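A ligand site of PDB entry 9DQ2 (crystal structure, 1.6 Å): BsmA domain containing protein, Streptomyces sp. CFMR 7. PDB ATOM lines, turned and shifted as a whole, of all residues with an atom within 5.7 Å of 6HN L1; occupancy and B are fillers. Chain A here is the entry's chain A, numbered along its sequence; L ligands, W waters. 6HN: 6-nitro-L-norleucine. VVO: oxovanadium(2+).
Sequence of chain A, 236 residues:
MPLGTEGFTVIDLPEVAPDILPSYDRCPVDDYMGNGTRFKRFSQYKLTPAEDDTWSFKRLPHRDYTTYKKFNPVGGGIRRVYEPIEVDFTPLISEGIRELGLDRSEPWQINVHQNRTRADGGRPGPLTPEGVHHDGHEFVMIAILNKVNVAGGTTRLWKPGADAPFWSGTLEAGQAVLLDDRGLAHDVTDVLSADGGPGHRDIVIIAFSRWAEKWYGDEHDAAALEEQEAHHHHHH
Water W1 lies within hydrogen-bond range of O of 6HN L1 (2.7 Å), ND2 of Asn 115 (2.8 Å) and NZ of Lys 40 (2.8 Å).
An oxygen (O1) of 6HN L1 sits at hydrogen-bond distance from the side-chain hydroxyl (OH) of Tyr 65, 2.6 Å away.
NE2 of His 137 is in hydrogen-bond range of O1 of 6HN L1, 2.7 Å away.
The side-chain amide nitrogen (ND2) of Asn 72 sits at hydrogen-bond distance from an oxygen (OXT) of 6HN L1, 2.8 Å away.
OE2 of Glu 130 lies within salt-bridge range of N of 6HN L1, 2.8 Å away.
O2 of 6HN L1 lies within hydrogen-bond range of NE2 of His 113.
The guanidinium group (NH1) of Arg 80 is in salt-bridge range of an oxygen (OXT) of 6HN L1 (2.9 Å).
An oxygen (O2) of 6HN L1 is in hydrogen-bond range of the side-chain amide nitrogen of Asn 111 (2.9 Å).
An oxygen (O) of 6HN L1 lies within salt-bridge range of the side-chain amino group of Lys 40, at 3.6 Å.
A vanadium atom (V1) of VVO L2 is bound by the side-chain carboxylate (OD1) of Asp 135.
NE2 of His 133 is bound to V1 of VVO L2 (2.2 Å).
O of Arg 80 lies within hydrogen-bond range of N of Tyr 65 (2.9 Å).
The side-chain amide nitrogen (ND2) of Asn 72 lies within hydrogen-bond range of the side-chain sulfur (SD) of Met 33, 3.8 Å away.
The backbone NH of Gly 75 lies within hydrogen-bond range of the side-chain amide oxygen of Asn 72 (2.8 Å).
NZ of Lys 40 sits close to ND1 of His 113, 3.2 Å away.
N of His 113 sits at hydrogen-bond distance from O of Ile 205 (2.9 Å).
The guanidinium group of Arg 80 sits at hydrogen-bond distance from the side-chain sulfur of Met 33, at 3.4 Å.
The guanidinium group (NH1) of Arg 80 sits at hydrogen-bond distance from the backbone carbonyl oxygen (O) of Gly 75 (3.0 Å).
The side-chain carboxylate of Asp 30 lies within hydrogen-bond range of the backbone NH of Met 33 (3.3 Å).
An oxygen (OXT) of 6HN L1 lies close to the side-chain sulfur of Met 33 (3.4 Å).
Residues that only touch 6HN L1: Asp 135 (3.5 Å), Ala 207 (3.6 Å), Trp 215 (3.7 Å) and Ile 205 (3.9 Å).
Hydrophobic or aromatic side chains that line 6HN L1: Met 33, Tyr 65, His 113, His 137, Ile 205, Ala 207 and Trp 215.
13 residues have an atom within 4 Å of 6HN L1: Met 33, Lys 40, Tyr 65, Asn 72, Arg 80, Asn 111, His 113, Glu 130, Asp 135, His 137, Ile 205, Ala 207 and Trp 215.
The nearest printed residue that does not touch 6HN L1 is Arg 38 (4.1 Å).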
ATOM      1  N   ASP A  30      -3.555 -25.533 -11.836  1.00  0.00           N
ATOM      2  CA  ASP A  30      -3.401 -26.288 -10.588  1.00  0.00           C
ATOM      3  C   ASP A  30      -4.354 -27.473 -10.631  1.00  0.00           C
ATOM      4  O   ASP A  30      -5.575 -27.276 -10.624  1.00  0.00           O
ATOM      5  CB  ASP A  30      -3.703 -25.365  -9.421  1.00  0.00           C
ATOM      6  CG  ASP A  30      -3.465 -25.977  -8.038  1.00  0.00           C
ATOM      7  OD1 ASP A  30      -3.337 -27.226  -7.900  1.00  0.00           O
ATOM      8  OD2 ASP A  30      -3.406 -25.155  -7.097  1.00  0.00           O
ATOM      9  N   MET A  33      -6.351 -27.929  -6.706  1.00  0.00           N
ATOM     10  CA  MET A  33      -7.161 -26.957  -6.002  1.00  0.00           C
ATOM     11  C   MET A  33      -7.765 -25.975  -6.989  1.00  0.00           C
ATOM     12  O   MET A  33      -7.179 -25.686  -8.040  1.00  0.00           O
ATOM     13  CB  MET A  33      -6.352 -26.199  -4.955  1.00  0.00           C
ATOM     14  CG  MET A  33      -5.921 -27.096  -3.832  1.00  0.00           C
ATOM     15  SD  MET A  33      -5.313 -26.191  -2.426  1.00  0.00           S
ATOM     16  CE  MET A  33      -6.802 -25.451  -1.753  1.00  0.00           C
ATOM     17  N   ARG A  38      -7.568 -22.002 -10.938  1.00  0.00           N
ATOM     18  CA  ARG A  38      -6.275 -21.631 -10.361  1.00  0.00           C
ATOM     19  C   ARG A  38      -5.115 -22.167 -11.207  1.00  0.00           C
ATOM     20  O   ARG A  38      -5.192 -23.286 -11.753  1.00  0.00           O
ATOM     21  CB  ARG A  38      -6.177 -22.170  -8.926  1.00  0.00           C
ATOM     22  CG  ARG A  38      -4.986 -21.650  -8.164  1.00  0.00           C
ATOM     23  CD  ARG A  38      -5.030 -22.164  -6.734  1.00  0.00           C
ATOM     24  NE  ARG A  38      -6.185 -21.632  -6.041  1.00  0.00           N
ATOM     25  CZ  ARG A  38      -6.318 -21.689  -4.731  1.00  0.00           C
ATOM     26  NH1 ARG A  38      -5.410 -22.306  -3.980  1.00  0.00           N
ATOM     27  NH2 ARG A  38      -7.388 -21.132  -4.146  1.00  0.00           N
ATOM     28  N   LYS A  40      -0.655 -22.274 -11.121  1.00  0.00           N
ATOM     29  CA  LYS A  40       0.336 -22.261 -10.040  1.00  0.00           C
ATOM     30  C   LYS A  40       1.718 -22.695 -10.539  1.00  0.00           C
ATOM     31  O   LYS A  40       1.819 -23.569 -11.395  1.00  0.00           O
ATOM     32  CB  LYS A  40      -0.107 -23.223  -8.922  1.00  0.00           C
ATOM     33  CG  LYS A  40       0.812 -23.351  -7.746  1.00  0.00           C
ATOM     34  CD  LYS A  40       0.079 -24.179  -6.700  1.00  0.00           C
ATOM     35  CE  LYS A  40       0.472 -23.825  -5.323  1.00  0.00           C
ATOM     36  NZ  LYS A  40      -0.420 -22.731  -4.860  1.00  0.00           N
ATOM     37  N   PHE A  42       5.579 -23.423  -8.163  1.00  0.00           N
ATOM     38  CA  PHE A  42       5.947 -23.642  -6.760  1.00  0.00           C
ATOM     39  C   PHE A  42       7.428 -23.872  -6.642  1.00  0.00           C
ATOM     40  O   PHE A  42       7.978 -24.705  -7.360  1.00  0.00           O
ATOM     41  CB  PHE A  42       5.193 -24.876  -6.235  1.00  0.00           C
ATOM     42  CG  PHE A  42       5.628 -25.346  -4.856  1.00  0.00           C
ATOM     43  CD1 PHE A  42       5.271 -24.646  -3.683  1.00  0.00           C
ATOM     44  CD2 PHE A  42       6.316 -26.542  -4.711  1.00  0.00           C
ATOM     45  CE1 PHE A  42       5.668 -25.181  -2.408  1.00  0.00           C
ATOM     46  CE2 PHE A  42       6.695 -27.041  -3.445  1.00  0.00           C
ATOM     47  CZ  PHE A  42       6.357 -26.371  -2.326  1.00  0.00           C
ATOM     48  N   TYR A  65       4.830 -30.572  -3.569  1.00  0.00           N
ATOM     49  CA  TYR A  65       4.312 -29.875  -2.392  1.00  0.00           C
ATOM     50  C   TYR A  65       3.475 -30.843  -1.579  1.00  0.00           C
ATOM     51  O   TYR A  65       2.631 -31.549  -2.124  1.00  0.00           O
ATOM     52  CB  TYR A  65       3.455 -28.683  -2.812  1.00  0.00           C
ATOM     53  CG  TYR A  65       2.776 -27.984  -1.661  1.00  0.00           C
ATOM     54  CD1 TYR A  65       3.502 -27.481  -0.589  1.00  0.00           C
ATOM     55  CD2 TYR A  65       1.396 -27.757  -1.683  1.00  0.00           C
ATOM     56  CE1 TYR A  65       2.866 -26.821   0.494  1.00  0.00           C
ATOM     57  CE2 TYR A  65       0.766 -27.086  -0.620  1.00  0.00           C
ATOM     58  CZ  TYR A  65       1.505 -26.627   0.450  1.00  0.00           C
ATOM     59  OH  TYR A  65       0.832 -25.994   1.466  1.00  0.00           O
ATOM     60  N   THR A  66       3.684 -30.861  -0.268  1.00  0.00           N
ATOM     61  CA  THR A  66       2.856 -31.671   0.630  1.00  0.00           C
ATOM     62  C   THR A  66       2.472 -30.809   1.827  1.00  0.00           C
ATOM     63  O   THR A  66       3.302 -30.092   2.399  1.00  0.00           O
ATOM     64  CB  THR A  66       3.573 -32.954   1.102  1.00  0.00           C
ATOM     65  OG1 THR A  66       4.794 -32.590   1.767  1.00  0.00           O
ATOM     66  CG2 THR A  66       3.911 -33.854  -0.090  1.00  0.00           C
ATOM     67  N   THR A  67       1.175 -30.840   2.177  1.00  0.00           N
ATOM     68  CA  THR A  67       0.749 -30.207   3.415  1.00  0.00           C
ATOM     69  C   THR A  67      -0.169 -31.169   4.167  1.00  0.00           C
ATOM     70  O   THR A  67      -0.423 -32.284   3.726  1.00  0.00           O
ATOM     71  CB  THR A  67       0.065 -28.852   3.158  1.00  0.00           C
ATOM     72  OG1 THR A  67      -0.258 -28.260   4.414  1.00  0.00           O
ATOM     73  CG2 THR A  67      -1.227 -28.985   2.344  1.00  0.00           C
ATOM     74  N   ASN A  72      -5.186 -27.977   5.904  1.00  0.00           N
ATOM     75  CA  ASN A  72      -5.812 -27.799   4.603  1.00  0.00           C
ATOM     76  C   ASN A  72      -6.592 -29.068   4.299  1.00  0.00           C
ATOM     77  O   ASN A  72      -6.047 -30.038   3.762  1.00  0.00           O
ATOM     78  CB  ASN A  72      -4.763 -27.526   3.524  1.00  0.00           C
ATOM     79  CG  ASN A  72      -5.378 -27.292   2.156  1.00  0.00           C
ATOM     80  OD1 ASN A  72      -6.552 -27.582   1.926  1.00  0.00           O
ATOM     81  ND2 ASN A  72      -4.573 -26.739   1.244  1.00  0.00           N
ATOM     82  N   GLY A  75      -6.745 -29.796   0.255  1.00  0.00           N
ATOM     83  CA  GLY A  75      -5.537 -30.034  -0.515  1.00  0.00           C
ATOM     84  C   GLY A  75      -4.418 -30.663   0.264  1.00  0.00           C
ATOM     85  O   GLY A  75      -3.277 -30.713  -0.214  1.00  0.00           O
ATOM     86  N   ARG A  80       1.499 -33.092  -4.343  1.00  0.00           N
ATOM     87  CA  ARG A  80       1.006 -32.141  -5.342  1.00  0.00           C
ATOM     88  C   ARG A  80       2.171 -31.763  -6.242  1.00  0.00           C
ATOM     89  O   ARG A  80       3.107 -31.070  -5.819  1.00  0.00           O
ATOM     90  CB  ARG A  80       0.383 -30.922  -4.669  1.00  0.00           C
ATOM     91  CG  ARG A  80      -0.963 -31.305  -4.057  1.00  0.00           C
ATOM     92  CD  ARG A  80      -1.459 -30.364  -2.988  1.00  0.00           C
ATOM     93  NE  ARG A  80      -1.715 -29.040  -3.557  1.00  0.00           N
ATOM     94  CZ  ARG A  80      -2.070 -27.990  -2.822  1.00  0.00           C
ATOM     95  NH1 ARG A  80      -2.391 -28.122  -1.535  1.00  0.00           N
ATOM     96  NH2 ARG A  80      -2.089 -26.781  -3.375  1.00  0.00           N
ATOM     97  N   TYR A  82       3.947 -29.839  -8.928  1.00  0.00           N
ATOM     98  CA  TYR A  82       3.887 -28.504  -9.527  1.00  0.00           C
ATOM     99  C   TYR A  82       5.183 -28.227 -10.291  1.00  0.00           C
ATOM    100  O   TYR A  82       6.238 -28.814 -10.007  1.00  0.00           O
ATOM    101  CB  TYR A  82       3.682 -27.421  -8.462  1.00  0.00           C
ATOM    102  CG  TYR A  82       2.318 -27.438  -7.850  1.00  0.00           C
ATOM    103  CD1 TYR A  82       1.161 -27.423  -8.652  1.00  0.00           C
ATOM    104  CD2 TYR A  82       2.162 -27.523  -6.479  1.00  0.00           C
ATOM    105  CE1 TYR A  82      -0.139 -27.463  -8.074  1.00  0.00           C
ATOM    106  CE2 TYR A  82       0.869 -27.557  -5.900  1.00  0.00           C
ATOM    107  CZ  TYR A  82      -0.250 -27.537  -6.705  1.00  0.00           C
ATOM    108  OH  TYR A  82      -1.471 -27.605  -6.126  1.00  0.00           O
ATOM    109  N   ASN A 111       8.352 -21.755   1.574  1.00  0.00           N
ATOM    110  CA  ASN A 111       7.557 -22.251   0.455  1.00  0.00           C
ATOM    111  C   ASN A 111       7.073 -21.024  -0.309  1.00  0.00           C
ATOM    112  O   ASN A 111       6.510 -20.103   0.293  1.00  0.00           O
ATOM    113  CB  ASN A 111       6.339 -23.042   0.942  1.00  0.00           C
ATOM    114  CG  ASN A 111       6.689 -24.403   1.444  1.00  0.00           C
ATOM    115  OD1 ASN A 111       7.837 -24.812   1.396  1.00  0.00           O
ATOM    116  ND2 ASN A 111       5.684 -25.109   1.999  1.00  0.00           N
ATOM    117  N   HIS A 113       4.607 -19.891  -3.443  1.00  0.00           N
ATOM    118  CA  HIS A 113       3.514 -20.263  -4.346  1.00  0.00           C
ATOM    119  C   HIS A 113       3.197 -19.100  -5.250  1.00  0.00           C
ATOM    120  O   HIS A 113       2.720 -18.048  -4.770  1.00  0.00           O
ATOM    121  CB  HIS A 113       2.259 -20.647  -3.559  1.00  0.00           C
ATOM    122  CG  HIS A 113       2.451 -21.756  -2.577  1.00  0.00           C
ATOM    123  ND1 HIS A 113       1.962 -23.029  -2.793  1.00  0.00           N
ATOM    124  CD2 HIS A 113       3.061 -21.801  -1.368  1.00  0.00           C
ATOM    125  CE1 HIS A 113       2.270 -23.808  -1.775  1.00  0.00           C
ATOM    126  NE2 HIS A 113       2.940 -23.086  -0.889  1.00  0.00           N
ATOM    127  N   ASN A 115       0.632 -17.892  -7.724  1.00  0.00           N
ATOM    128  CA  ASN A 115      -0.766 -18.254  -8.036  1.00  0.00           C
ATOM    129  C   ASN A 115      -1.454 -17.224  -8.903  1.00  0.00           C
ATOM    130  O   ASN A 115      -1.355 -16.004  -8.645  1.00  0.00           O
ATOM    131  CB  ASN A 115      -1.634 -18.377  -6.770  1.00  0.00           C
ATOM    132  CG  ASN A 115      -1.384 -19.636  -5.942  1.00  0.00           C
ATOM    133  OD1 ASN A 115      -0.348 -20.292  -6.025  1.00  0.00           O
ATOM    134  ND2 ASN A 115      -2.353 -19.916  -5.051  1.00  0.00           N
ATOM    135  N   GLU A 130     -10.251 -23.920   1.845  1.00  0.00           N
ATOM    136  CA  GLU A 130      -9.985 -24.394   3.197  1.00  0.00           C
ATOM    137  C   GLU A 130     -10.922 -23.768   4.226  1.00  0.00           C
ATOM    138  O   GLU A 130     -11.073 -24.319   5.327  1.00  0.00           O
ATOM    139  CB  GLU A 130      -8.525 -24.068   3.610  1.00  0.00           C
ATOM    140  CG  GLU A 130      -7.394 -24.529   2.655  1.00  0.00           C
ATOM    141  CD  GLU A 130      -7.003 -23.499   1.588  1.00  0.00           C
ATOM    142  OE1 GLU A 130      -7.843 -22.675   1.209  1.00  0.00           O
ATOM    143  OE2 GLU A 130      -5.835 -23.474   1.106  1.00  0.00           O
ATOM    144  N   HIS A 133      -8.549 -20.568   8.219  1.00  0.00           N
ATOM    145  CA  HIS A 133      -7.516 -21.577   8.480  1.00  0.00           C
ATOM    146  C   HIS A 133      -6.242 -20.922   8.974  1.00  0.00           C
ATOM    147  O   HIS A 133      -6.004 -19.712   8.790  1.00  0.00           O
ATOM    148  CB  HIS A 133      -7.189 -22.398   7.223  1.00  0.00           C
ATOM    149  CG  HIS A 133      -6.610 -21.572   6.122  1.00  0.00           C
ATOM    150  ND1 HIS A 133      -7.401 -20.763   5.311  1.00  0.00           N
ATOM    151  CD2 HIS A 133      -5.335 -21.390   5.706  1.00  0.00           C
ATOM    152  CE1 HIS A 133      -6.631 -20.147   4.435  1.00  0.00           C
ATOM    153  NE2 HIS A 133      -5.377 -20.498   4.662  1.00  0.00           N
ATOM    154  N   ASP A 135      -2.191 -21.689   7.998  1.00  0.00           N
ATOM    155  CA  ASP A 135      -1.373 -22.443   7.020  1.00  0.00           C
ATOM    156  C   ASP A 135      -0.521 -23.524   7.672  1.00  0.00           C
ATOM    157  O   ASP A 135      -0.129 -24.471   6.984  1.00  0.00           O
ATOM    158  CB  ASP A 135      -0.428 -21.522   6.237  1.00  0.00           C
ATOM    159  CG  ASP A 135      -1.110 -20.670   5.187  1.00  0.00           C
ATOM    160  OD1 ASP A 135      -2.353 -20.585   5.204  1.00  0.00           O
ATOM    161  OD2 ASP A 135      -0.383 -20.084   4.337  1.00  0.00           O
ATOM    162  N   HIS A 137       2.387 -22.696   9.363  1.00  0.00           N
ATOM    163  CA  HIS A 137       3.734 -22.163   9.456  1.00  0.00           C
ATOM    164  C   HIS A 137       3.794 -21.109  10.564  1.00  0.00           C
ATOM    165  O   HIS A 137       2.827 -20.878  11.296  1.00  0.00           O
ATOM    166  CB  HIS A 137       4.162 -21.574   8.113  1.00  0.00           C
ATOM    167  CG  HIS A 137       4.169 -22.565   6.981  1.00  0.00           C
ATOM    168  ND1 HIS A 137       5.323 -23.138   6.500  1.00  0.00           N
ATOM    169  CD2 HIS A 137       3.162 -23.048   6.215  1.00  0.00           C
ATOM    170  CE1 HIS A 137       5.034 -23.954   5.517  1.00  0.00           C
ATOM    171  NE2 HIS A 137       3.723 -23.917   5.317  1.00  0.00           N
ATOM    172  N   ILE A 205       2.426 -16.281  -2.501  1.00  0.00           N
ATOM    173  CA  ILE A 205       2.299 -16.598  -1.083  1.00  0.00           C
ATOM    174  C   ILE A 205       3.616 -17.184  -0.616  1.00  0.00           C
ATOM    175  O   ILE A 205       4.174 -18.080  -1.253  1.00  0.00           O
ATOM    176  CB  ILE A 205       1.178 -17.618  -0.845  1.00  0.00           C
ATOM    177  CG1 ILE A 205      -0.136 -17.081  -1.429  1.00  0.00           C
ATOM    178  CG2 ILE A 205       1.030 -17.918   0.638  1.00  0.00           C
ATOM    179  CD1 ILE A 205      -1.135 -18.195  -1.637  1.00  0.00           C
ATOM    180  N   ALA A 207       5.422 -18.853   2.717  1.00  0.00           N
ATOM    181  CA  ALA A 207       5.204 -19.417   4.041  1.00  0.00           C
ATOM    182  C   ALA A 207       6.570 -19.644   4.681  1.00  0.00           C
ATOM    183  O   ALA A 207       7.426 -20.322   4.084  1.00  0.00           O
ATOM    184  CB  ALA A 207       4.422 -20.740   3.951  1.00  0.00           C
ATOM    185  N   TRP A 215       9.321 -27.427   6.078  1.00  0.00           N
ATOM    186  CA  TRP A 215       8.301 -28.152   5.320  1.00  0.00           C
ATOM    187  C   TRP A 215       8.898 -28.715   4.050  1.00  0.00           C
ATOM    188  O   TRP A 215       8.443 -28.465   2.933  1.00  0.00           O
ATOM    189  CB  TRP A 215       7.156 -27.195   5.030  1.00  0.00           C
ATOM    190  CG  TRP A 215       6.278 -26.921   6.201  1.00  0.00           C
ATOM    191  CD1 TRP A 215       6.624 -26.485   7.453  1.00  0.00           C
ATOM    192  CD2 TRP A 215       4.847 -27.046   6.202  1.00  0.00           C
ATOM    193  NE1 TRP A 215       5.480 -26.350   8.241  1.00  0.00           N
ATOM    194  CE2 TRP A 215       4.385 -26.691   7.478  1.00  0.00           C
ATOM    195  CE3 TRP A 215       3.922 -27.445   5.227  1.00  0.00           C
ATOM    196  CZ2 TRP A 215       3.010 -26.710   7.819  1.00  0.00           C
ATOM    197  CZ3 TRP A 215       2.565 -27.451   5.560  1.00  0.00           C
ATOM    198  CH2 TRP A 215       2.132 -27.099   6.833  1.00  0.00           C
HETATM  199  N1  6HN L   1       2.345 -23.686   2.546  1.00  0.00           N
HETATM  200  N   6HN L   1      -3.029 -23.476   1.320  1.00  0.00           N
HETATM  201  CA  6HN L   1      -2.279 -23.168   0.097  1.00  0.00           C
HETATM  202  C   6HN L   1      -2.438 -24.355  -0.862  1.00  0.00           C
HETATM  203  OXT 6HN L   1      -2.722 -25.488  -0.398  1.00  0.00           O
HETATM  204  O   6HN L   1      -2.252 -24.185  -2.092  1.00  0.00           O
HETATM  205  CB  6HN L   1      -0.775 -23.024   0.378  1.00  0.00           C
HETATM  206  CG  6HN L   1      -0.474 -21.747   1.150  1.00  0.00           C
HETATM  207  CD  6HN L   1       0.989 -21.716   1.613  1.00  0.00           C
HETATM  208  CE  6HN L   1       1.199 -22.780   2.686  1.00  0.00           C
HETATM  209  O2  6HN L   1       3.303 -23.437   1.884  1.00  0.00           O
HETATM  210  O1  6HN L   1       2.334 -24.732   3.133  1.00  0.00           O
HETATM  211  O1  VVO L   2      -3.498 -20.722   2.606  1.00  0.00           O
HETATM  212  V1  VVO L   2      -3.587 -19.553   3.748  1.00  0.00           V
HETATM  213  O   HOH W   1      -2.000 -21.588  -2.875  1.00  0.00           O
HETATM  214  O   HOH W   2      -3.199 -24.035  -4.672  1.00  0.00           O
